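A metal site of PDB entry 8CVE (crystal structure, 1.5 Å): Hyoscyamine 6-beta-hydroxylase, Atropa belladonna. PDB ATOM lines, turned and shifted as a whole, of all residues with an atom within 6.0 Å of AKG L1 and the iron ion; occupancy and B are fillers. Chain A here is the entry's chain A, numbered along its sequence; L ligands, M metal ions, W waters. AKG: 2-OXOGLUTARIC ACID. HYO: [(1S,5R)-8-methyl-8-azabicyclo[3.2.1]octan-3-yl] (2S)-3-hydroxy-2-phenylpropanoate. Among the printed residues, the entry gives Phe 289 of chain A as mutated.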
ATOM      1  N   LYS A 129     -15.464  21.326  22.007  1.00  0.00           N
ATOM      2  CA  LYS A 129     -14.781  22.458  22.667  1.00  0.00           C
ATOM      3  C   LYS A 129     -15.820  23.336  23.379  1.00  0.00           C
ATOM      4  O   LYS A 129     -16.873  23.588  22.790  1.00  0.00           O
ATOM      5  CB  LYS A 129     -14.036  23.283  21.618  1.00  0.00           C
ATOM      6  CG  LYS A 129     -13.408  24.585  22.095  1.00  0.00           C
ATOM      7  CD  LYS A 129     -12.444  25.177  21.087  1.00  0.00           C
ATOM      8  CE  LYS A 129     -13.120  25.794  19.884  1.00  0.00           C
ATOM      9  NZ  LYS A 129     -13.795  27.077  20.217  1.00  0.00           N
ATOM     10  N   LEU A 198      -9.164  33.749  24.946  1.00  0.00           N
ATOM     11  CA  LEU A 198     -10.002  32.536  24.748  1.00  0.00           C
ATOM     12  C   LEU A 198      -9.388  31.414  25.587  1.00  0.00           C
ATOM     13  O   LEU A 198      -8.249  31.003  25.287  1.00  0.00           O
ATOM     14  CB  LEU A 198     -10.044  32.179  23.259  1.00  0.00           C
ATOM     15  CG  LEU A 198     -11.092  32.917  22.434  1.00  0.00           C
ATOM     16  CD1 LEU A 198     -10.807  34.408  22.386  1.00  0.00           C
ATOM     17  CD2 LEU A 198     -11.167  32.342  21.032  1.00  0.00           C
ATOM     18  N   ASN A 200      -9.816  27.654  26.239  1.00  0.00           N
ATOM     19  CA  ASN A 200     -10.434  26.516  25.511  1.00  0.00           C
ATOM     20  C   ASN A 200     -10.419  25.288  26.421  1.00  0.00           C
ATOM     21  O   ASN A 200      -9.351  24.966  26.935  1.00  0.00           O
ATOM     22  CB  ASN A 200      -9.705  26.218  24.211  1.00  0.00           C
ATOM     23  CG  ASN A 200      -9.654  27.419  23.304  1.00  0.00           C
ATOM     24  OD1 ASN A 200     -10.697  27.992  22.981  1.00  0.00           O
ATOM     25  ND2 ASN A 200      -8.465  27.818  22.896  1.00  0.00           N
ATOM     26  N   TYR A 202     -11.305  21.267  26.258  1.00  0.00           N
ATOM     27  CA  TYR A 202     -11.522  20.055  25.430  1.00  0.00           C
ATOM     28  C   TYR A 202     -11.770  18.881  26.367  1.00  0.00           C
ATOM     29  O   TYR A 202     -10.816  18.295  26.884  1.00  0.00           O
ATOM     30  CB  TYR A 202     -10.308  19.820  24.523  1.00  0.00           C
ATOM     31  CG  TYR A 202      -9.894  21.020  23.718  1.00  0.00           C
ATOM     32  CD1 TYR A 202     -10.474  21.287  22.488  1.00  0.00           C
ATOM     33  CD2 TYR A 202      -8.927  21.888  24.184  1.00  0.00           C
ATOM     34  CE1 TYR A 202     -10.090  22.389  21.740  1.00  0.00           C
ATOM     35  CE2 TYR A 202      -8.536  22.993  23.448  1.00  0.00           C
ATOM     36  CZ  TYR A 202      -9.124  23.246  22.225  1.00  0.00           C
ATOM     37  OH  TYR A 202      -8.731  24.341  21.499  1.00  0.00           O
ATOM     38  N   SER A 214     -10.898  21.621  17.399  1.00  0.00           N
ATOM     39  CA  SER A 214     -10.885  22.883  16.622  1.00  0.00           C
ATOM     40  C   SER A 214     -10.563  22.535  15.174  1.00  0.00           C
ATOM     41  O   SER A 214      -9.518  21.903  14.947  1.00  0.00           O
ATOM     42  CB  SER A 214      -9.879  23.844  17.217  1.00  0.00           C
ATOM     43  OG  SER A 214     -10.239  25.197  16.959  1.00  0.00           O
ATOM     44  N   HIS A 217      -7.718  26.136  10.757  1.00  0.00           N
ATOM     45  CA  HIS A 217      -7.970  27.587  10.573  1.00  0.00           C
ATOM     46  C   HIS A 217      -6.659  28.366  10.667  1.00  0.00           C
ATOM     47  O   HIS A 217      -5.744  27.917  11.373  1.00  0.00           O
ATOM     48  CB  HIS A 217      -8.968  28.096  11.623  1.00  0.00           C
ATOM     49  CG  HIS A 217      -8.468  28.047  13.029  1.00  0.00           C
ATOM     50  ND1 HIS A 217      -8.411  26.866  13.747  1.00  0.00           N
ATOM     51  CD2 HIS A 217      -7.978  29.003  13.857  1.00  0.00           C
ATOM     52  CE1 HIS A 217      -7.929  27.099  14.945  1.00  0.00           C
ATOM     53  NE2 HIS A 217      -7.650  28.405  15.044  1.00  0.00           N
ATOM     54  N   TYR A 218      -6.618  29.533  10.022  1.00  0.00           N
ATOM     55  CA  TYR A 218      -5.807  30.683  10.466  1.00  0.00           C
ATOM     56  C   TYR A 218      -6.542  31.355  11.620  1.00  0.00           C
ATOM     57  O   TYR A 218      -7.788  31.404  11.578  1.00  0.00           O
ATOM     58  CB  TYR A 218      -5.680  31.772   9.401  1.00  0.00           C
ATOM     59  CG  TYR A 218      -4.913  31.437   8.148  1.00  0.00           C
ATOM     60  CD1 TYR A 218      -3.526  31.531   8.101  1.00  0.00           C
ATOM     61  CD2 TYR A 218      -5.575  31.076   6.991  1.00  0.00           C
ATOM     62  CE1 TYR A 218      -2.824  31.267   6.942  1.00  0.00           C
ATOM     63  CE2 TYR A 218      -4.889  30.805   5.818  1.00  0.00           C
ATOM     64  CZ  TYR A 218      -3.505  30.888   5.799  1.00  0.00           C
ATOM     65  OH  TYR A 218      -2.816  30.629   4.638  1.00  0.00           O
ATOM     66  N   ASP A 219      -5.810  31.915  12.573  1.00  0.00           N
ATOM     67  CA  ASP A 219      -6.347  32.979  13.454  1.00  0.00           C
ATOM     68  C   ASP A 219      -6.510  34.222  12.574  1.00  0.00           C
ATOM     69  O   ASP A 219      -5.549  34.567  11.884  1.00  0.00           O
ATOM     70  CB  ASP A 219      -5.440  33.193  14.676  1.00  0.00           C
ATOM     71  CG  ASP A 219      -5.367  32.022  15.655  1.00  0.00           C
ATOM     72  OD1 ASP A 219      -6.183  31.058  15.534  1.00  0.00           O
ATOM     73  OD2 ASP A 219      -4.514  32.091  16.543  1.00  0.00           O
ATOM     74  N   THR A 224      -1.357  35.728  17.786  1.00  0.00           N
ATOM     75  CA  THR A 224      -1.962  34.994  18.925  1.00  0.00           C
ATOM     76  C   THR A 224      -0.838  34.319  19.701  1.00  0.00           C
ATOM     77  O   THR A 224       0.022  33.692  19.062  1.00  0.00           O
ATOM     78  CB  THR A 224      -2.974  33.956  18.435  1.00  0.00           C
ATOM     79  OG1 THR A 224      -4.004  34.638  17.713  1.00  0.00           O
ATOM     80  CG2 THR A 224      -3.606  33.178  19.575  1.00  0.00           C
ATOM     81  N   LEU A 226      -0.334  31.377  22.524  1.00  0.00           N
ATOM     82  CA  LEU A 226      -1.085  30.186  22.986  1.00  0.00           C
ATOM     83  C   LEU A 226      -0.266  29.507  24.082  1.00  0.00           C
ATOM     84  O   LEU A 226       0.928  29.239  23.858  1.00  0.00           O
ATOM     85  CB  LEU A 226      -1.331  29.282  21.775  1.00  0.00           C
ATOM     86  CG  LEU A 226      -2.113  27.989  22.005  1.00  0.00           C
ATOM     87  CD1 LEU A 226      -1.266  26.907  22.653  1.00  0.00           C
ATOM     88  CD2 LEU A 226      -3.368  28.228  22.810  1.00  0.00           C
ATOM     89  N   GLN A 228      -0.127  26.097  26.445  1.00  0.00           N
ATOM     90  CA  GLN A 228      -0.634  24.710  26.493  1.00  0.00           C
ATOM     91  C   GLN A 228       0.277  23.861  27.381  1.00  0.00           C
ATOM     92  O   GLN A 228       1.493  24.146  27.433  1.00  0.00           O
ATOM     93  CB  GLN A 228      -0.732  24.114  25.084  1.00  0.00           C
ATOM     94  CG  GLN A 228       0.580  24.148  24.315  1.00  0.00           C
ATOM     95  CD  GLN A 228       0.583  23.239  23.099  1.00  0.00           C
ATOM     96  OE1 GLN A 228      -0.389  22.543  22.810  1.00  0.00           O
ATOM     97  NE2 GLN A 228       1.692  23.244  22.383  1.00  0.00           N
ATOM     98  N   GLY A 232      -2.275  18.033  21.454  1.00  0.00           N
ATOM     99  CA  GLY A 232      -3.547  18.182  20.715  1.00  0.00           C
ATOM    100  C   GLY A 232      -3.446  19.218  19.620  1.00  0.00           C
ATOM    101  O   GLY A 232      -4.226  19.125  18.664  1.00  0.00           O
ATOM    102  N   LEU A 233      -2.520  20.184  19.746  1.00  0.00           N
ATOM    103  CA  LEU A 233      -2.345  21.240  18.720  1.00  0.00           C
ATOM    104  C   LEU A 233      -1.543  20.661  17.548  1.00  0.00           C
ATOM    105  O   LEU A 233      -0.482  20.051  17.779  1.00  0.00           O
ATOM    106  CB  LEU A 233      -1.620  22.443  19.324  1.00  0.00           C
ATOM    107  CG  LEU A 233      -1.308  23.588  18.357  1.00  0.00           C
ATOM    108  CD1 LEU A 233      -2.584  24.203  17.790  1.00  0.00           C
ATOM    109  CD2 LEU A 233      -0.452  24.640  19.040  1.00  0.00           C
ATOM    110  N   ASN A 255       1.344  32.225  17.008  1.00  0.00           N
ATOM    111  CA  ASN A 255       0.614  31.965  15.741  1.00  0.00           C
ATOM    112  C   ASN A 255       0.453  33.297  15.012  1.00  0.00           C
ATOM    113  O   ASN A 255      -0.229  34.168  15.557  1.00  0.00           O
ATOM    114  CB  ASN A 255      -0.762  31.336  15.994  1.00  0.00           C
ATOM    115  CG  ASN A 255      -0.738  29.857  16.330  1.00  0.00           C
ATOM    116  OD1 ASN A 255      -0.115  29.068  15.624  1.00  0.00           O
ATOM    117  ND2 ASN A 255      -1.445  29.458  17.371  1.00  0.00           N
ATOM    118  N   HIS A 273      -3.694  25.812  11.725  1.00  0.00           N
ATOM    119  CA  HIS A 273      -3.602  24.835  12.838  1.00  0.00           C
ATOM    120  C   HIS A 273      -4.987  24.301  13.190  1.00  0.00           C
ATOM    121  O   HIS A 273      -5.996  24.909  12.805  1.00  0.00           O
ATOM    122  CB  HIS A 273      -2.882  25.457  14.040  1.00  0.00           C
ATOM    123  CG  HIS A 273      -3.488  26.748  14.483  1.00  0.00           C
ATOM    124  ND1 HIS A 273      -3.153  27.962  13.918  1.00  0.00           N
ATOM    125  CD2 HIS A 273      -4.422  27.012  15.424  1.00  0.00           C
ATOM    126  CE1 HIS A 273      -3.867  28.918  14.494  1.00  0.00           C
ATOM    127  NE2 HIS A 273      -4.637  28.362  15.426  1.00  0.00           N
ATOM    128  N   ARG A 274      -5.014  23.172  13.892  1.00  0.00           N
ATOM    129  CA  ARG A 274      -6.247  22.508  14.381  1.00  0.00           C
ATOM    130  C   ARG A 274      -5.933  21.884  15.748  1.00  0.00           C
ATOM    131  O   ARG A 274      -4.748  21.802  16.113  1.00  0.00           O
ATOM    132  CB  ARG A 274      -6.730  21.455  13.382  1.00  0.00           C
ATOM    133  CG  ARG A 274      -5.890  20.189  13.365  1.00  0.00           C
ATOM    134  CD  ARG A 274      -6.309  19.227  12.275  1.00  0.00           C
ATOM    135  NE  ARG A 274      -5.494  18.027  12.340  1.00  0.00           N
ATOM    136  CZ  ARG A 274      -5.444  17.075  11.398  1.00  0.00           C
ATOM    137  NH1 ARG A 274      -6.179  17.172  10.304  1.00  0.00           N
ATOM    138  NH2 ARG A 274      -4.657  16.038  11.563  1.00  0.00           N
ATOM    139  N   VAL A 275      -6.974  21.452  16.454  1.00  0.00           N
ATOM    140  CA  VAL A 275      -6.831  20.725  17.743  1.00  0.00           C
ATOM    141  C   VAL A 275      -7.605  19.410  17.634  1.00  0.00           C
ATOM    142  O   VAL A 275      -8.785  19.439  17.245  1.00  0.00           O
ATOM    143  CB  VAL A 275      -7.311  21.567  18.928  1.00  0.00           C
ATOM    144  CG1 VAL A 275      -7.177  20.793  20.242  1.00  0.00           C
ATOM    145  CG2 VAL A 275      -6.565  22.891  19.001  1.00  0.00           C
ATOM    146  N   ARG A 283      -8.269  18.787  28.418  1.00  0.00           N
ATOM    147  CA  ARG A 283      -7.167  19.701  28.034  1.00  0.00           C
ATOM    148  C   ARG A 283      -7.691  21.130  28.115  1.00  0.00           C
ATOM    149  O   ARG A 283      -8.814  21.376  27.634  1.00  0.00           O
ATOM    150  CB  ARG A 283      -6.674  19.403  26.619  1.00  0.00           C
ATOM    151  CG  ARG A 283      -5.596  20.349  26.108  1.00  0.00           C
ATOM    152  CD  ARG A 283      -5.018  19.827  24.807  1.00  0.00           C
ATOM    153  NE  ARG A 283      -4.006  20.713  24.256  1.00  0.00           N
ATOM    154  CZ  ARG A 283      -4.242  21.787  23.500  1.00  0.00           C
ATOM    155  NH1 ARG A 283      -5.486  22.126  23.204  1.00  0.00           N
ATOM    156  NH2 ARG A 283      -3.235  22.510  23.057  1.00  0.00           N
ATOM    157  N   SER A 285      -6.362  25.062  27.065  1.00  0.00           N
ATOM    158  CA  SER A 285      -5.380  25.968  26.426  1.00  0.00           C
ATOM    159  C   SER A 285      -5.840  27.403  26.636  1.00  0.00           C
ATOM    160  O   SER A 285      -7.056  27.639  26.781  1.00  0.00           O
ATOM    161  CB  SER A 285      -5.179  25.645  24.974  1.00  0.00           C
ATOM    162  OG  SER A 285      -6.325  25.966  24.206  1.00  0.00           O
ATOM    163  N   ALA A 287      -5.432  31.109  24.864  1.00  0.00           N
ATOM    164  CA  ALA A 287      -5.051  31.805  23.620  1.00  0.00           C
ATOM    165  C   ALA A 287      -5.343  33.297  23.779  1.00  0.00           C
ATOM    166  O   ALA A 287      -6.511  33.641  24.037  1.00  0.00           O
ATOM    167  CB  ALA A 287      -5.788  31.207  22.446  1.00  0.00           C
ATOM    168  N   PHE A 289      -5.584  36.540  21.730  1.00  0.00           N
ATOM    169  CA  PHE A 289      -5.829  37.008  20.345  1.00  0.00           C
ATOM    170  C   PHE A 289      -5.672  38.532  20.311  1.00  0.00           C
ATOM    171  O   PHE A 289      -6.574  39.236  20.771  1.00  0.00           O
ATOM    172  CB  PHE A 289      -7.233  36.620  19.902  1.00  0.00           C
ATOM    173  CG  PHE A 289      -7.364  35.188  19.435  1.00  0.00           C
ATOM    174  CD1 PHE A 289      -7.332  34.140  20.333  1.00  0.00           C
ATOM    175  CD2 PHE A 289      -7.512  34.918  18.083  1.00  0.00           C
ATOM    176  CE1 PHE A 289      -7.448  32.832  19.869  1.00  0.00           C
ATOM    177  CE2 PHE A 289      -7.631  33.609  17.629  1.00  0.00           C
ATOM    178  CZ  PHE A 289      -7.584  32.578  18.531  1.00  0.00           C
HETATM  179  C1  AKG L   1      -7.649  28.793  18.986  1.00  0.00           C
HETATM  180  O1  AKG L   1      -7.781  29.463  17.962  1.00  0.00           O
HETATM  181  O2  AKG L   1      -8.332  28.999  20.000  1.00  0.00           O
HETATM  182  C2  AKG L   1      -6.751  27.843  18.977  1.00  0.00           C
HETATM  183  O5  AKG L   1      -6.149  27.625  17.912  1.00  0.00           O
HETATM  184  C3  AKG L   1      -6.424  27.029  20.208  1.00  0.00           C
HETATM  185  C4  AKG L   1      -5.384  25.951  19.984  1.00  0.00           C
HETATM  186  C5  AKG L   1      -5.150  25.000  21.152  1.00  0.00           C
HETATM  187  O3  AKG L   1      -4.003  24.555  21.303  1.00  0.00           O
HETATM  188  O4  AKG L   1      -6.113  24.687  21.885  1.00  0.00           O
HETATM  189  C10 HYO L   2     -12.857  31.824  17.407  1.00  0.00           C
HETATM  190  C13 HYO L   2     -12.122  34.857  16.899  1.00  0.00           C
HETATM  191  C15 HYO L   2     -11.348  36.806  15.661  1.00  0.00           C
HETATM  192  C17 HYO L   2     -10.294  37.112  14.804  1.00  0.00           C
HETATM  193  C20 HYO L   2     -12.816  38.145  14.297  1.00  0.00           C
HETATM  194  C21 HYO L   2     -11.762  38.450  13.440  1.00  0.00           C
HETATM  195  C05 HYO L   2     -11.154  30.719  15.408  1.00  0.00           C
HETATM  196  C06 HYO L   2     -11.757  30.786  17.612  1.00  0.00           C
HETATM  197  C07 HYO L   2      -9.959  31.370  16.113  1.00  0.00           C
HETATM  198  C08 HYO L   2     -10.383  31.438  17.586  1.00  0.00           C
HETATM  199  C09 HYO L   2     -12.209  31.718  14.963  1.00  0.00           C
HETATM  200  C11 HYO L   2     -12.706  32.607  16.097  1.00  0.00           C
HETATM  201  C12 HYO L   2     -11.011  28.661  16.679  1.00  0.00           C
HETATM  202  C14 HYO L   2     -11.093  35.950  16.852  1.00  0.00           C
HETATM  203  C16 HYO L   2     -11.098  36.805  18.115  1.00  0.00           C
HETATM  204  C18 HYO L   2     -12.611  37.332  15.398  1.00  0.00           C
HETATM  205  C19 HYO L   2     -10.500  37.934  13.694  1.00  0.00           C
HETATM  206  N04 HYO L   2     -11.781  29.888  16.442  1.00  0.00           N
HETATM  207  O01 HYO L   2     -11.737  33.646  16.238  1.00  0.00           O
HETATM  208  O02 HYO L   2     -13.216  34.953  17.440  1.00  0.00           O
HETATM  209  O03 HYO L   2     -10.114  37.847  17.982  1.00  0.00           O
HETATM  210 FE    FE M   1      -6.273  29.246  16.496  1.00  0.00          FE
HETATM  211  O   HOH W   1      -9.634  26.088  19.413  1.00  0.00           O
HETATM  212  O   HOH W   2      -4.575  29.973  18.052  1.00  0.00           O
HETATM  213  O   HOH W   3     -11.109  28.692  20.374  1.00  0.00           O
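Of the 21 residues printed, 3 come within 4 Å of the iron ion.
The iron ion is bound by the side-chain carboxylate (OD1) of Asp 219, an oxygen (O1) of AKG L1, a ring nitrogen (NE2) of His 273, an oxygen (O5) of AKG L1, a ring nitrogen (NE2) of His 217 and water W2.
Leu 226 touches AKG L1.
CB of Leu 233 touches O3 of AKG L1 (3.7 Å).
Val 275 touches AKG L1 (CG2 to C5, 3.3 Å).
Phe 289 touches AKG L1.
Hydrophobic or aromatic side chains within 4 Å of AKG L1: Tyr 202, His 217, Leu 226, Leu 233, His 273, Val 275 and Phe 289.
The nearest printed residue that does not touch AKG L1 is Ala 287 (4.2 Å).
Water W2 lies within hydrogen-bond range of OD2 of Asp 219 (2.6 Å) and ND2 of Asn 255 (3.2 Å).
Water W3 lies within hydrogen-bond range of the side-chain amide oxygen (OD1) of Asn 200 (2.7 Å), an oxygen (O2) of AKG L1 (2.8 Å) and the side-chain amino group (NZ) of Lys 129 (3.1 Å).
Water W1 lies within hydrogen-bond range of OG of Ser 214, OH of Tyr 202 and O2 of AKG L1.
OD2 of Asp 219 is in hydrogen-bond range of OG1 of Thr 224, 2.8 Å away.
The backbone carbonyl oxygen of Ser 285 sits at hydrogen-bond distance from the backbone NH of Asn 200 (2.8 Å).
The backbone carbonyl oxygen of Arg 283 sits at hydrogen-bond distance from the backbone NH of Tyr 202, at 2.8 Å.
OE1 of Gln 228 is in hydrogen-bond range of NH2 of Arg 283 (2.9 Å).
The backbone NH (N) of Val 275 sits at hydrogen-bond distance from the backbone carbonyl oxygen (O) of Ser 214 (3.0 Å).
O4 of AKG L1 lies within hydrogen-bond range of OG of Ser 285, 2.7 Å away.
The side-chain hydroxyl (OH) of Tyr 202 lies within hydrogen-bond range of an oxygen (O4) of AKG L1, at 2.7 Å.
NH2 of Arg 283 is in salt-bridge range of O3 of AKG L1 (2.8 Å).
ND2 of Asn 200 sits at hydrogen-bond distance from O2 of AKG L1 (3.1 Å).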
